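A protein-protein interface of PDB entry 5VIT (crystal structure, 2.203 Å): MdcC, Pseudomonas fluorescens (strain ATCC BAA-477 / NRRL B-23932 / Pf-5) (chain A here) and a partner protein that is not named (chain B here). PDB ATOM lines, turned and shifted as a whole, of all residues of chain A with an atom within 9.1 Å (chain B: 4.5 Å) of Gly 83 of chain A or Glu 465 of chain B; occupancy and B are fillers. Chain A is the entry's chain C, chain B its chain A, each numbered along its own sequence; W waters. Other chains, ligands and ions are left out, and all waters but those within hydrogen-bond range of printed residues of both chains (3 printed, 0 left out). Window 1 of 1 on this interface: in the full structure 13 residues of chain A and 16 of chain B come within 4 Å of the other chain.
Gly 83 of chain A touches just these residues of chain B: Glu 422 and Glu 465.
Printed residues of chain A within 4 Å of Glu 422 of chain B: Thr 81 (2.4 Å), Gly 83 (3.6 Å) and Val 84 (3.8 Å).
Of the printed residues of chain A, Val 236 of chain B touches Leu 87.
Asp 27 of chain A touches none of the printed residues of chain B.
The nearest printed residue of chain B that does not touch Gly 83 of chain A is Thr 423 of chain B (4.7 Å).
The nearest residue of chain A that does not touch Glu 465 of chain B is Pro 82 of chain A (4.8 Å).
The nearest printed residue of chain B that does not touch Leu 87 of chain A is Leu 239 of chain B (4.03 Å).
Of the 11 printed residues of chain B, 5 touch a printed residue of chain A.
Of the 20 printed residues of chain A, 6 touch a printed residue of chain B.
Printed residues of chain A that touch a printed residue of chain B: Thr 81, Gly 83, Val 84, Arg 86, Leu 87 and Glu 90.
Among the printed residues, 9 pairs touch across the chains.
Among the printed residues, Asp or Glu carboxylates within 4 Å of a Lys or Arg side-chain nitrogen of the other chain: Arg 86 of chain A with Glu 466 of chain B and Glu 90 of chain A with Arg 521 of chain B.
O of Glu 465 of chain B is in hydrogen-bond range of NH2 of Arg 521 of chain B (2.8 Å).
NE of Arg 86 of chain A is in salt-bridge range of OE2 of Glu 90 of chain A.
The side-chain hydroxyl (OG1) of Thr 81 of chain A sits at hydrogen-bond distance from the backbone NH (N) of Val 84 of chain A (3.2 Å).
OG1 of Thr 423 of chain B sits at hydrogen-bond distance from OE2 of Glu 465 of chain B, 2.5 Å away.
The side-chain sulfur (SD) of Met 240 of chain B lies close to the backbone NH (N) of Glu 465 of chain B, at 3.6 Å.
OE2 of Glu 466 of chain B is in salt-bridge range of NH1 of Arg 86 of chain A.
The guanidinium group (NH1) of Arg 521 of chain B sits close to the guanidinium group (NH2) of Arg 86 of chain A.
The side-chain carboxylate of Glu 422 of chain B sits at hydrogen-bond distance from the side-chain hydroxyl of Thr 81 of chain A (2.4 Å).
The side-chain carboxylate (OE1) of Glu 90 of chain A is in salt-bridge range of the guanidinium group (NE) of Arg 521 of chain B, 3.6 Å away.
CA of Gly 83 of chain A touches OE1 of Glu 422 of chain B, 3.6 Å away.
Gly 83 of chain A touches Glu 465 of chain B (CA to OE2, 3.4 Å).
Glu 422 of chain B touches Val 84 of chain A.
N of Val 236 of chain B touches CD2 of Leu 87 of chain A, at 3.7 Å.
Leu 87 of chain A touches Arg 521 of chain B (CD1 to O, 3.7 Å).
Water W3 lies within hydrogen-bond range of O of Glu 466 of chain B (2.6 Å), NH1 of Arg 521 of chain B (3.2 Å) and NH1 of Arg 86 of chain A (3.3 Å).
Water W2 bridges the side-chain carboxylate of Glu 422 of chain B (2.6 Å) and the side-chain hydroxyl of Thr 81 of chain A (3.3 Å).
Water W1 lies within hydrogen-bond range of OE1 of Glu 422 of chain B (2.8 Å), OG1 of Thr 423 of chain B (2.9 Å), N of Gly 83 of chain A (2.9 Å) and OE2 of Glu 465 of chain B (3.0 Å).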
ATOM      1  N   GLY A  26     -16.334 -12.386 -22.948  1.00  0.00           N
ATOM      2  CA  GLY A  26     -17.759 -12.490 -22.699  1.00  0.00           C
ATOM      3  C   GLY A  26     -18.102 -13.691 -21.842  1.00  0.00           C
ATOM      4  O   GLY A  26     -19.263 -14.095 -21.748  1.00  0.00           O
ATOM      5  N   ASP A  27     -17.086 -14.261 -21.209  1.00  0.00           N
ATOM      6  CA  ASP A  27     -17.264 -15.462 -20.391  1.00  0.00           C
ATOM      7  C   ASP A  27     -16.384 -15.385 -19.141  1.00  0.00           C
ATOM      8  O   ASP A  27     -15.602 -14.446 -18.988  1.00  0.00           O
ATOM      9  CB  ASP A  27     -16.938 -16.725 -21.215  1.00  0.00           C
ATOM     10  CG  ASP A  27     -17.579 -17.982 -20.646  1.00  0.00           C
ATOM     11  OD1 ASP A  27     -17.405 -19.067 -21.250  1.00  0.00           O
ATOM     12  OD2 ASP A  27     -18.248 -17.895 -19.594  1.00  0.00           O
ATOM     13  N   LEU A  28     -16.511 -16.374 -18.259  1.00  0.00           N
ATOM     14  CA  LEU A  28     -15.696 -16.437 -17.046  1.00  0.00           C
ATOM     15  C   LEU A  28     -15.466 -17.888 -16.655  1.00  0.00           C
ATOM     16  O   LEU A  28     -16.245 -18.764 -17.036  1.00  0.00           O
ATOM     17  CB  LEU A  28     -16.375 -15.696 -15.886  1.00  0.00           C
ATOM     18  CG  LEU A  28     -17.593 -16.392 -15.262  1.00  0.00           C
ATOM     19  CD1 LEU A  28     -17.927 -15.770 -13.920  1.00  0.00           C
ATOM     20  CD2 LEU A  28     -18.854 -16.353 -16.207  1.00  0.00           C
ATOM     21  N   ARG A  54     -21.881  -3.929  -8.884  1.00  0.00           N
ATOM     22  CA  ARG A  54     -22.574  -4.902  -9.710  1.00  0.00           C
ATOM     23  C   ARG A  54     -22.346  -6.329  -9.162  1.00  0.00           C
ATOM     24  O   ARG A  54     -23.302  -7.065  -8.926  1.00  0.00           O
ATOM     25  CB  ARG A  54     -22.105  -4.780 -11.165  1.00  0.00           C
ATOM     26  CG  ARG A  54     -22.672  -5.823 -12.099  1.00  0.00           C
ATOM     27  CD  ARG A  54     -21.986  -5.780 -13.474  1.00  0.00           C
ATOM     28  NE  ARG A  54     -22.639  -4.861 -14.412  1.00  0.00           N
ATOM     29  CZ  ARG A  54     -22.257  -3.607 -14.651  1.00  0.00           C
ATOM     30  NH1 ARG A  54     -21.196  -3.096 -14.025  1.00  0.00           N
ATOM     31  NH2 ARG A  54     -22.932  -2.868 -15.530  1.00  0.00           N
ATOM     32  N   TRP A  55     -21.084  -6.699  -8.936  1.00  0.00           N
ATOM     33  CA  TRP A  55     -20.760  -8.023  -8.410  1.00  0.00           C
ATOM     34  C   TRP A  55     -21.364  -8.216  -7.011  1.00  0.00           C
ATOM     35  O   TRP A  55     -21.835  -9.302  -6.667  1.00  0.00           O
ATOM     36  CB  TRP A  55     -19.239  -8.239  -8.378  1.00  0.00           C
ATOM     37  CG  TRP A  55     -18.625  -8.516  -9.739  1.00  0.00           C
ATOM     38  CD1 TRP A  55     -18.054  -7.605 -10.581  1.00  0.00           C
ATOM     39  CD2 TRP A  55     -18.548  -9.783 -10.415  1.00  0.00           C
ATOM     40  NE1 TRP A  55     -17.614  -8.222 -11.728  1.00  0.00           N
ATOM     41  CE2 TRP A  55     -17.907  -9.558 -11.652  1.00  0.00           C
ATOM     42  CE3 TRP A  55     -18.950 -11.080 -10.094  1.00  0.00           C
ATOM     43  CZ2 TRP A  55     -17.665 -10.583 -12.565  1.00  0.00           C
ATOM     44  CZ3 TRP A  55     -18.704 -12.096 -10.996  1.00  0.00           C
ATOM     45  CH2 TRP A  55     -18.068 -11.844 -12.214  1.00  0.00           C
ATOM     46  N   LEU A  58     -25.080  -9.001  -7.415  1.00  0.00           N
ATOM     47  CA  LEU A  58     -25.216 -10.340  -7.979  1.00  0.00           C
ATOM     48  C   LEU A  58     -25.159 -11.412  -6.878  1.00  0.00           C
ATOM     49  O   LEU A  58     -26.068 -12.253  -6.743  1.00  0.00           O
ATOM     50  CB  LEU A  58     -24.114 -10.545  -9.027  1.00  0.00           C
ATOM     51  CG  LEU A  58     -24.226 -11.657 -10.065  1.00  0.00           C
ATOM     52  CD1 LEU A  58     -25.651 -11.841 -10.459  1.00  0.00           C
ATOM     53  CD2 LEU A  58     -23.428 -11.278 -11.296  1.00  0.00           C
ATOM     54  N   ARG A  61     -28.078 -11.350  -4.236  1.00  0.00           N
ATOM     55  CA  ARG A  61     -29.292 -12.009  -4.706  1.00  0.00           C
ATOM     56  C   ARG A  61     -29.149 -13.495  -4.721  1.00  0.00           C
ATOM     57  O   ARG A  61     -30.075 -14.235  -4.378  1.00  0.00           O
ATOM     58  CB  ARG A  61     -29.641 -11.533  -6.098  1.00  0.00           C
ATOM     59  CG  ARG A  61     -29.983 -10.087  -6.112  1.00  0.00           C
ATOM     60  CD  ARG A  61     -30.756  -9.797  -7.322  1.00  0.00           C
ATOM     61  NE  ARG A  61     -31.211  -8.422  -7.315  1.00  0.00           N
ATOM     62  CZ  ARG A  61     -32.052  -7.944  -8.216  1.00  0.00           C
ATOM     63  NH1 ARG A  61     -32.512  -8.764  -9.153  1.00  0.00           N
ATOM     64  NH2 ARG A  61     -32.428  -6.669  -8.170  1.00  0.00           N
ATOM     65  N   GLY A  79     -15.488 -10.199 -18.922  1.00  0.00           N
ATOM     66  CA  GLY A  79     -16.630  -9.420 -19.389  1.00  0.00           C
ATOM     67  C   GLY A  79     -17.936 -10.154 -19.656  1.00  0.00           C
ATOM     68  O   GLY A  79     -18.716  -9.757 -20.522  1.00  0.00           O
ATOM     69  N   ALA A  80     -18.188 -11.226 -18.915  1.00  0.00           N
ATOM     70  CA  ALA A  80     -19.457 -11.917 -19.005  1.00  0.00           C
ATOM     71  C   ALA A  80     -20.601 -10.990 -18.554  1.00  0.00           C
ATOM     72  O   ALA A  80     -20.395 -10.139 -17.697  1.00  0.00           O
ATOM     73  CB  ALA A  80     -19.425 -13.177 -18.167  1.00  0.00           C
ATOM     74  N   THR A  81     -21.793 -11.146 -19.134  1.00  0.00           N
ATOM     75  CA  THR A  81     -22.968 -10.456 -18.611  1.00  0.00           C
ATOM     76  C   THR A  81     -23.312 -11.032 -17.233  1.00  0.00           C
ATOM     77  O   THR A  81     -22.942 -12.165 -16.925  1.00  0.00           O
ATOM     78  CB  THR A  81     -24.179 -10.610 -19.536  1.00  0.00           C
ATOM     79  OG1 THR A  81     -24.470 -12.008 -19.696  1.00  0.00           O
ATOM     80  CG2 THR A  81     -23.904  -9.974 -20.891  1.00  0.00           C
ATOM     81  N   PRO A  82     -24.026 -10.259 -16.399  1.00  0.00           N
ATOM     82  CA  PRO A  82     -24.484 -10.756 -15.097  1.00  0.00           C
ATOM     83  C   PRO A  82     -25.309 -12.020 -15.235  1.00  0.00           C
ATOM     84  O   PRO A  82     -25.249 -12.898 -14.372  1.00  0.00           O
ATOM     85  CB  PRO A  82     -25.336  -9.605 -14.571  1.00  0.00           C
ATOM     86  CG  PRO A  82     -24.680  -8.411 -15.143  1.00  0.00           C
ATOM     87  CD  PRO A  82     -24.300  -8.821 -16.550  1.00  0.00           C
ATOM     88  N   GLY A  83     -26.070 -12.104 -16.324  1.00  0.00           N
ATOM     89  CA  GLY A  83     -26.809 -13.307 -16.649  1.00  0.00           C
ATOM     90  C   GLY A  83     -25.926 -14.529 -16.827  1.00  0.00           C
ATOM     91  O   GLY A  83     -26.198 -15.584 -16.246  1.00  0.00           O
ATOM     92  N   VAL A  84     -24.870 -14.397 -17.628  1.00  0.00           N
ATOM     93  CA  VAL A  84     -23.921 -15.498 -17.807  1.00  0.00           C
ATOM     94  C   VAL A  84     -23.217 -15.822 -16.484  1.00  0.00           C
ATOM     95  O   VAL A  84     -23.078 -16.990 -16.128  1.00  0.00           O
ATOM     96  CB  VAL A  84     -22.866 -15.178 -18.893  1.00  0.00           C
ATOM     97  CG1 VAL A  84     -21.742 -16.236 -18.911  1.00  0.00           C
ATOM     98  CG2 VAL A  84     -23.534 -15.072 -20.269  1.00  0.00           C
ATOM     99  N   VAL A  85     -22.793 -14.782 -15.760  1.00  0.00           N
ATOM    100  CA  VAL A  85     -22.136 -14.961 -14.464  1.00  0.00           C
ATOM    101  C   VAL A  85     -23.021 -15.765 -13.495  1.00  0.00           C
ATOM    102  O   VAL A  85     -22.586 -16.770 -12.926  1.00  0.00           O
ATOM    103  CB  VAL A  85     -21.779 -13.603 -13.798  1.00  0.00           C
ATOM    104  CG1 VAL A  85     -21.224 -13.837 -12.416  1.00  0.00           C
ATOM    105  CG2 VAL A  85     -20.794 -12.804 -14.649  1.00  0.00           C
ATOM    106  N   ARG A  86     -24.263 -15.325 -13.321  1.00  0.00           N
ATOM    107  CA  ARG A  86     -25.193 -16.028 -12.442  1.00  0.00           C
ATOM    108  C   ARG A  86     -25.351 -17.506 -12.824  1.00  0.00           C
ATOM    109  O   ARG A  86     -25.260 -18.386 -11.971  1.00  0.00           O
ATOM    110  CB  ARG A  86     -26.563 -15.349 -12.447  1.00  0.00           C
ATOM    111  CG  ARG A  86     -27.567 -16.152 -11.652  1.00  0.00           C
ATOM    112  CD  ARG A  86     -28.913 -15.480 -11.488  1.00  0.00           C
ATOM    113  NE  ARG A  86     -29.810 -16.413 -10.817  1.00  0.00           N
ATOM    114  CZ  ARG A  86     -31.114 -16.224 -10.655  1.00  0.00           C
ATOM    115  NH1 ARG A  86     -31.708 -15.131 -11.130  1.00  0.00           N
ATOM    116  NH2 ARG A  86     -31.826 -17.143 -10.023  1.00  0.00           N
ATOM    117  N   LEU A  87     -25.567 -17.768 -14.115  1.00  0.00           N
ATOM    118  CA  LEU A  87     -25.767 -19.131 -14.603  1.00  0.00           C
ATOM    119  C   LEU A  87     -24.572 -20.047 -14.300  1.00  0.00           C
ATOM    120  O   LEU A  87     -24.743 -21.178 -13.852  1.00  0.00           O
ATOM    121  CB  LEU A  87     -26.046 -19.106 -16.105  1.00  0.00           C
ATOM    122  CG  LEU A  87     -26.648 -20.371 -16.708  1.00  0.00           C
ATOM    123  CD1 LEU A  87     -27.959 -20.739 -15.998  1.00  0.00           C
ATOM    124  CD2 LEU A  87     -26.874 -20.173 -18.201  1.00  0.00           C
ATOM    125  N   ARG A  88     -23.364 -19.551 -14.540  1.00  0.00           N
ATOM    126  CA  ARG A  88     -22.153 -20.311 -14.240  1.00  0.00           C
ATOM    127  C   ARG A  88     -21.915 -20.576 -12.765  1.00  0.00           C
ATOM    128  O   ARG A  88     -21.460 -21.656 -12.392  1.00  0.00           O
ATOM    129  CB  ARG A  88     -20.943 -19.596 -14.800  1.00  0.00           C
ATOM    130  CG  ARG A  88     -20.842 -19.853 -16.256  1.00  0.00           C
ATOM    131  CD  ARG A  88     -19.444 -19.706 -16.690  1.00  0.00           C
ATOM    132  NE  ARG A  88     -19.082 -20.726 -17.652  1.00  0.00           N
ATOM    133  CZ  ARG A  88     -19.486 -20.752 -18.909  1.00  0.00           C
ATOM    134  NH1 ARG A  88     -20.312 -19.813 -19.356  1.00  0.00           N
ATOM    135  NH2 ARG A  88     -19.064 -21.726 -19.717  1.00  0.00           N
ATOM    136  N   LEU A  89     -22.213 -19.577 -11.938  1.00  0.00           N
ATOM    137  CA  LEU A  89     -22.081 -19.724 -10.504  1.00  0.00           C
ATOM    138  C   LEU A  89     -23.030 -20.810 -10.029  1.00  0.00           C
ATOM    139  O   LEU A  89     -22.678 -21.611  -9.161  1.00  0.00           O
ATOM    140  CB  LEU A  89     -22.353 -18.398  -9.796  1.00  0.00           C
ATOM    141  CG  LEU A  89     -21.132 -17.492  -9.678  1.00  0.00           C
ATOM    142  CD1 LEU A  89     -21.532 -16.067  -9.367  1.00  0.00           C
ATOM    143  CD2 LEU A  89     -20.250 -18.049  -8.581  1.00  0.00           C
ATOM    144  N   GLU A  90     -24.229 -20.851 -10.615  1.00  0.00           N
ATOM    145  CA  GLU A  90     -25.207 -21.870 -10.245  1.00  0.00           C
ATOM    146  C   GLU A  90     -24.738 -23.241 -10.741  1.00  0.00           C
ATOM    147  O   GLU A  90     -24.875 -24.236 -10.018  1.00  0.00           O
ATOM    148  CB  GLU A  90     -26.606 -21.504 -10.774  1.00  0.00           C
ATOM    149  CG  GLU A  90     -27.286 -20.379  -9.955  1.00  0.00           C
ATOM    150  CD  GLU A  90     -28.467 -19.693 -10.665  1.00  0.00           C
ATOM    151  OE1 GLU A  90     -28.450 -19.591 -11.917  1.00  0.00           O
ATOM    152  OE2 GLU A  90     -29.397 -19.220  -9.968  1.00  0.00           O
ATOM    153  N   GLN A  91     -24.151 -23.292 -11.941  1.00  0.00           N
ATOM    154  CA  GLN A  91     -23.530 -24.525 -12.448  1.00  0.00           C
ATOM    155  C   GLN A  91     -22.418 -25.051 -11.521  1.00  0.00           C
ATOM    156  O   GLN A  91     -22.304 -26.257 -11.267  1.00  0.00           O
ATOM    157  CB  GLN A  91     -22.934 -24.303 -13.838  1.00  0.00           C
ATOM    158  CG  GLN A  91     -23.933 -23.950 -14.935  1.00  0.00           C
ATOM    159  CD  GLN A  91     -23.255 -23.697 -16.289  1.00  0.00           C
ATOM    160  OE1 GLN A  91     -22.020 -23.565 -16.378  1.00  0.00           O
ATOM    161  NE2 GLN A  91     -24.067 -23.614 -17.347  1.00  0.00           N
ATOM    162  N   VAL B 236     -27.241 -19.181 -21.780  1.00  0.00           N
ATOM    163  CA  VAL B 236     -28.239 -18.187 -21.361  1.00  0.00           C
ATOM    164  C   VAL B 236     -29.341 -18.010 -22.431  1.00  0.00           C
ATOM    165  O   VAL B 236     -30.520 -17.847 -22.089  1.00  0.00           O
ATOM    166  CB  VAL B 236     -27.593 -16.813 -21.043  1.00  0.00           C
ATOM    167  CG1 VAL B 236     -26.881 -16.227 -22.260  1.00  0.00           C
ATOM    168  CG2 VAL B 236     -28.638 -15.846 -20.520  1.00  0.00           C
ATOM    169  N   LEU B 239     -31.647 -20.996 -22.116  1.00  0.00           N
ATOM    170  CA  LEU B 239     -32.504 -20.807 -20.951  1.00  0.00           C
ATOM    171  C   LEU B 239     -33.718 -19.932 -21.297  1.00  0.00           C
ATOM    172  O   LEU B 239     -34.853 -20.321 -21.021  1.00  0.00           O
ATOM    173  CB  LEU B 239     -31.724 -20.192 -19.791  1.00  0.00           C
ATOM    174  CG  LEU B 239     -32.510 -19.873 -18.509  1.00  0.00           C
ATOM    175  CD1 LEU B 239     -33.438 -21.017 -18.038  1.00  0.00           C
ATOM    176  CD2 LEU B 239     -31.525 -19.500 -17.408  1.00  0.00           C
ATOM    177  N   MET B 240     -33.483 -18.775 -21.916  1.00  0.00           N
ATOM    178  CA  MET B 240     -34.588 -17.913 -22.333  1.00  0.00           C
ATOM    179  C   MET B 240     -35.498 -18.648 -23.334  1.00  0.00           C
ATOM    180  O   MET B 240     -36.729 -18.594 -23.239  1.00  0.00           O
ATOM    181  CB  MET B 240     -34.048 -16.604 -22.932  1.00  0.00           C
ATOM    182  CG  MET B 240     -33.269 -15.771 -21.926  1.00  0.00           C
ATOM    183  SD  MET B 240     -32.850 -14.116 -22.507  1.00  0.00           S
ATOM    184  CE  MET B 240     -31.631 -14.415 -23.778  1.00  0.00           C
ATOM    185  N   VAL B 421     -34.997 -10.750 -24.158  1.00  0.00           N
ATOM    186  CA  VAL B 421     -33.701 -10.128 -24.121  1.00  0.00           C
ATOM    187  C   VAL B 421     -33.038 -10.382 -22.777  1.00  0.00           C
ATOM    188  O   VAL B 421     -33.713 -10.508 -21.748  1.00  0.00           O
ATOM    189  CB  VAL B 421     -33.843  -8.599 -24.409  1.00  0.00           C
ATOM    190  CG1 VAL B 421     -34.569  -7.892 -23.269  1.00  0.00           C
ATOM    191  CG2 VAL B 421     -32.515  -7.961 -24.702  1.00  0.00           C
ATOM    192  N   GLU B 422     -31.711 -10.481 -22.805  1.00  0.00           N
ATOM    193  CA  GLU B 422     -30.911 -10.590 -21.595  1.00  0.00           C
ATOM    194  C   GLU B 422     -30.955  -9.279 -20.811  1.00  0.00           C
ATOM    195  O   GLU B 422     -31.084  -8.197 -21.409  1.00  0.00           O
ATOM    196  CB  GLU B 422     -29.463 -10.953 -21.952  1.00  0.00           C
ATOM    197  CG  GLU B 422     -28.946 -12.061 -21.084  1.00  0.00           C
ATOM    198  CD  GLU B 422     -27.470 -12.323 -21.232  1.00  0.00           C
ATOM    199  OE1 GLU B 422     -26.829 -12.434 -20.176  1.00  0.00           O
ATOM    200  OE2 GLU B 422     -26.965 -12.466 -22.366  1.00  0.00           O
ATOM    201  N   THR B 423     -30.842  -9.357 -19.485  1.00  0.00           N
ATOM    202  CA  THR B 423     -30.906  -8.141 -18.674  1.00  0.00           C
ATOM    203  C   THR B 423     -29.781  -7.174 -18.980  1.00  0.00           C
ATOM    204  O   THR B 423     -29.908  -5.975 -18.719  1.00  0.00           O
ATOM    205  CB  THR B 423     -30.874  -8.440 -17.171  1.00  0.00           C
ATOM    206  OG1 THR B 423     -29.783  -9.314 -16.889  1.00  0.00           O
ATOM    207  CG2 THR B 423     -32.175  -9.106 -16.742  1.00  0.00           C
ATOM    208  N   THR B 464     -36.757 -12.718 -20.062  1.00  0.00           N
ATOM    209  CA  THR B 464     -35.401 -12.392 -19.661  1.00  0.00           C
ATOM    210  C   THR B 464     -34.733 -13.679 -19.122  1.00  0.00           C
ATOM    211  O   THR B 464     -35.439 -14.625 -18.829  1.00  0.00           O
ATOM    212  CB  THR B 464     -35.497 -11.252 -18.618  1.00  0.00           C
ATOM    213  OG1 THR B 464     -35.261  -9.966 -19.229  1.00  0.00           O
ATOM    214  CG2 THR B 464     -34.659 -11.478 -17.488  1.00  0.00           C
ATOM    215  N   GLU B 465     -33.408 -13.748 -18.983  1.00  0.00           N
ATOM    216  CA  GLU B 465     -32.807 -14.923 -18.327  1.00  0.00           C
ATOM    217  C   GLU B 465     -33.304 -15.122 -16.872  1.00  0.00           C
ATOM    218  O   GLU B 465     -33.174 -16.214 -16.320  1.00  0.00           O
ATOM    219  CB  GLU B 465     -31.264 -14.842 -18.352  1.00  0.00           C
ATOM    220  CG  GLU B 465     -30.596 -13.995 -17.261  1.00  0.00           C
ATOM    221  CD  GLU B 465     -30.538 -12.500 -17.571  1.00  0.00           C
ATOM    222  OE1 GLU B 465     -31.192 -12.047 -18.531  1.00  0.00           O
ATOM    223  OE2 GLU B 465     -29.828 -11.766 -16.852  1.00  0.00           O
ATOM    224  N   GLU B 466     -33.869 -14.077 -16.267  1.00  0.00           N
ATOM    225  CA  GLU B 466     -34.468 -14.128 -14.929  1.00  0.00           C
ATOM    226  C   GLU B 466     -35.856 -14.757 -14.891  1.00  0.00           C
ATOM    227  O   GLU B 466     -36.233 -15.402 -13.908  1.00  0.00           O
ATOM    228  CB  GLU B 466     -34.566 -12.721 -14.352  1.00  0.00           C
ATOM    229  CG  GLU B 466     -33.232 -12.021 -14.225  1.00  0.00           C
ATOM    230  CD  GLU B 466     -32.519 -12.405 -12.950  1.00  0.00           C
ATOM    231  OE1 GLU B 466     -33.169 -12.416 -11.886  1.00  0.00           O
ATOM    232  OE2 GLU B 466     -31.312 -12.694 -13.005  1.00  0.00           O
ATOM    233  N   GLY B 467     -36.629 -14.547 -15.953  1.00  0.00           N
ATOM    234  CA  GLY B 467     -37.993 -15.024 -15.975  1.00  0.00           C
ATOM    235  C   GLY B 467     -38.890 -14.271 -16.931  1.00  0.00           C
ATOM    236  O   GLY B 467     -38.441 -13.453 -17.739  1.00  0.00           O
ATOM    237  N   ARG B 521     -32.557 -24.071 -13.993  1.00  0.00           N
ATOM    238  CA  ARG B 521     -31.660 -23.179 -14.741  1.00  0.00           C
ATOM    239  C   ARG B 521     -30.427 -23.887 -15.303  1.00  0.00           C
ATOM    240  O   ARG B 521     -30.062 -23.686 -16.465  1.00  0.00           O
ATOM    241  CB  ARG B 521     -31.186 -22.017 -13.869  1.00  0.00           C
ATOM    242  CG  ARG B 521     -32.205 -21.491 -12.904  1.00  0.00           C
ATOM    243  CD  ARG B 521     -31.653 -20.284 -12.187  1.00  0.00           C
ATOM    244  NE  ARG B 521     -31.819 -19.115 -13.022  1.00  0.00           N
ATOM    245  CZ  ARG B 521     -32.807 -18.242 -12.865  1.00  0.00           C
ATOM    246  NH1 ARG B 521     -33.691 -18.389 -11.865  1.00  0.00           N
ATOM    247  NH2 ARG B 521     -32.900 -17.214 -13.700  1.00  0.00           N
HETATM  248  O   HOH W   1     -27.524 -10.479 -18.275  1.00  0.00           O
HETATM  249  O   HOH W   2     -24.442 -12.965 -22.899  1.00  0.00           O
HETATM  250  O   HOH W   3     -34.977 -15.517 -11.636  1.00  0.00           O
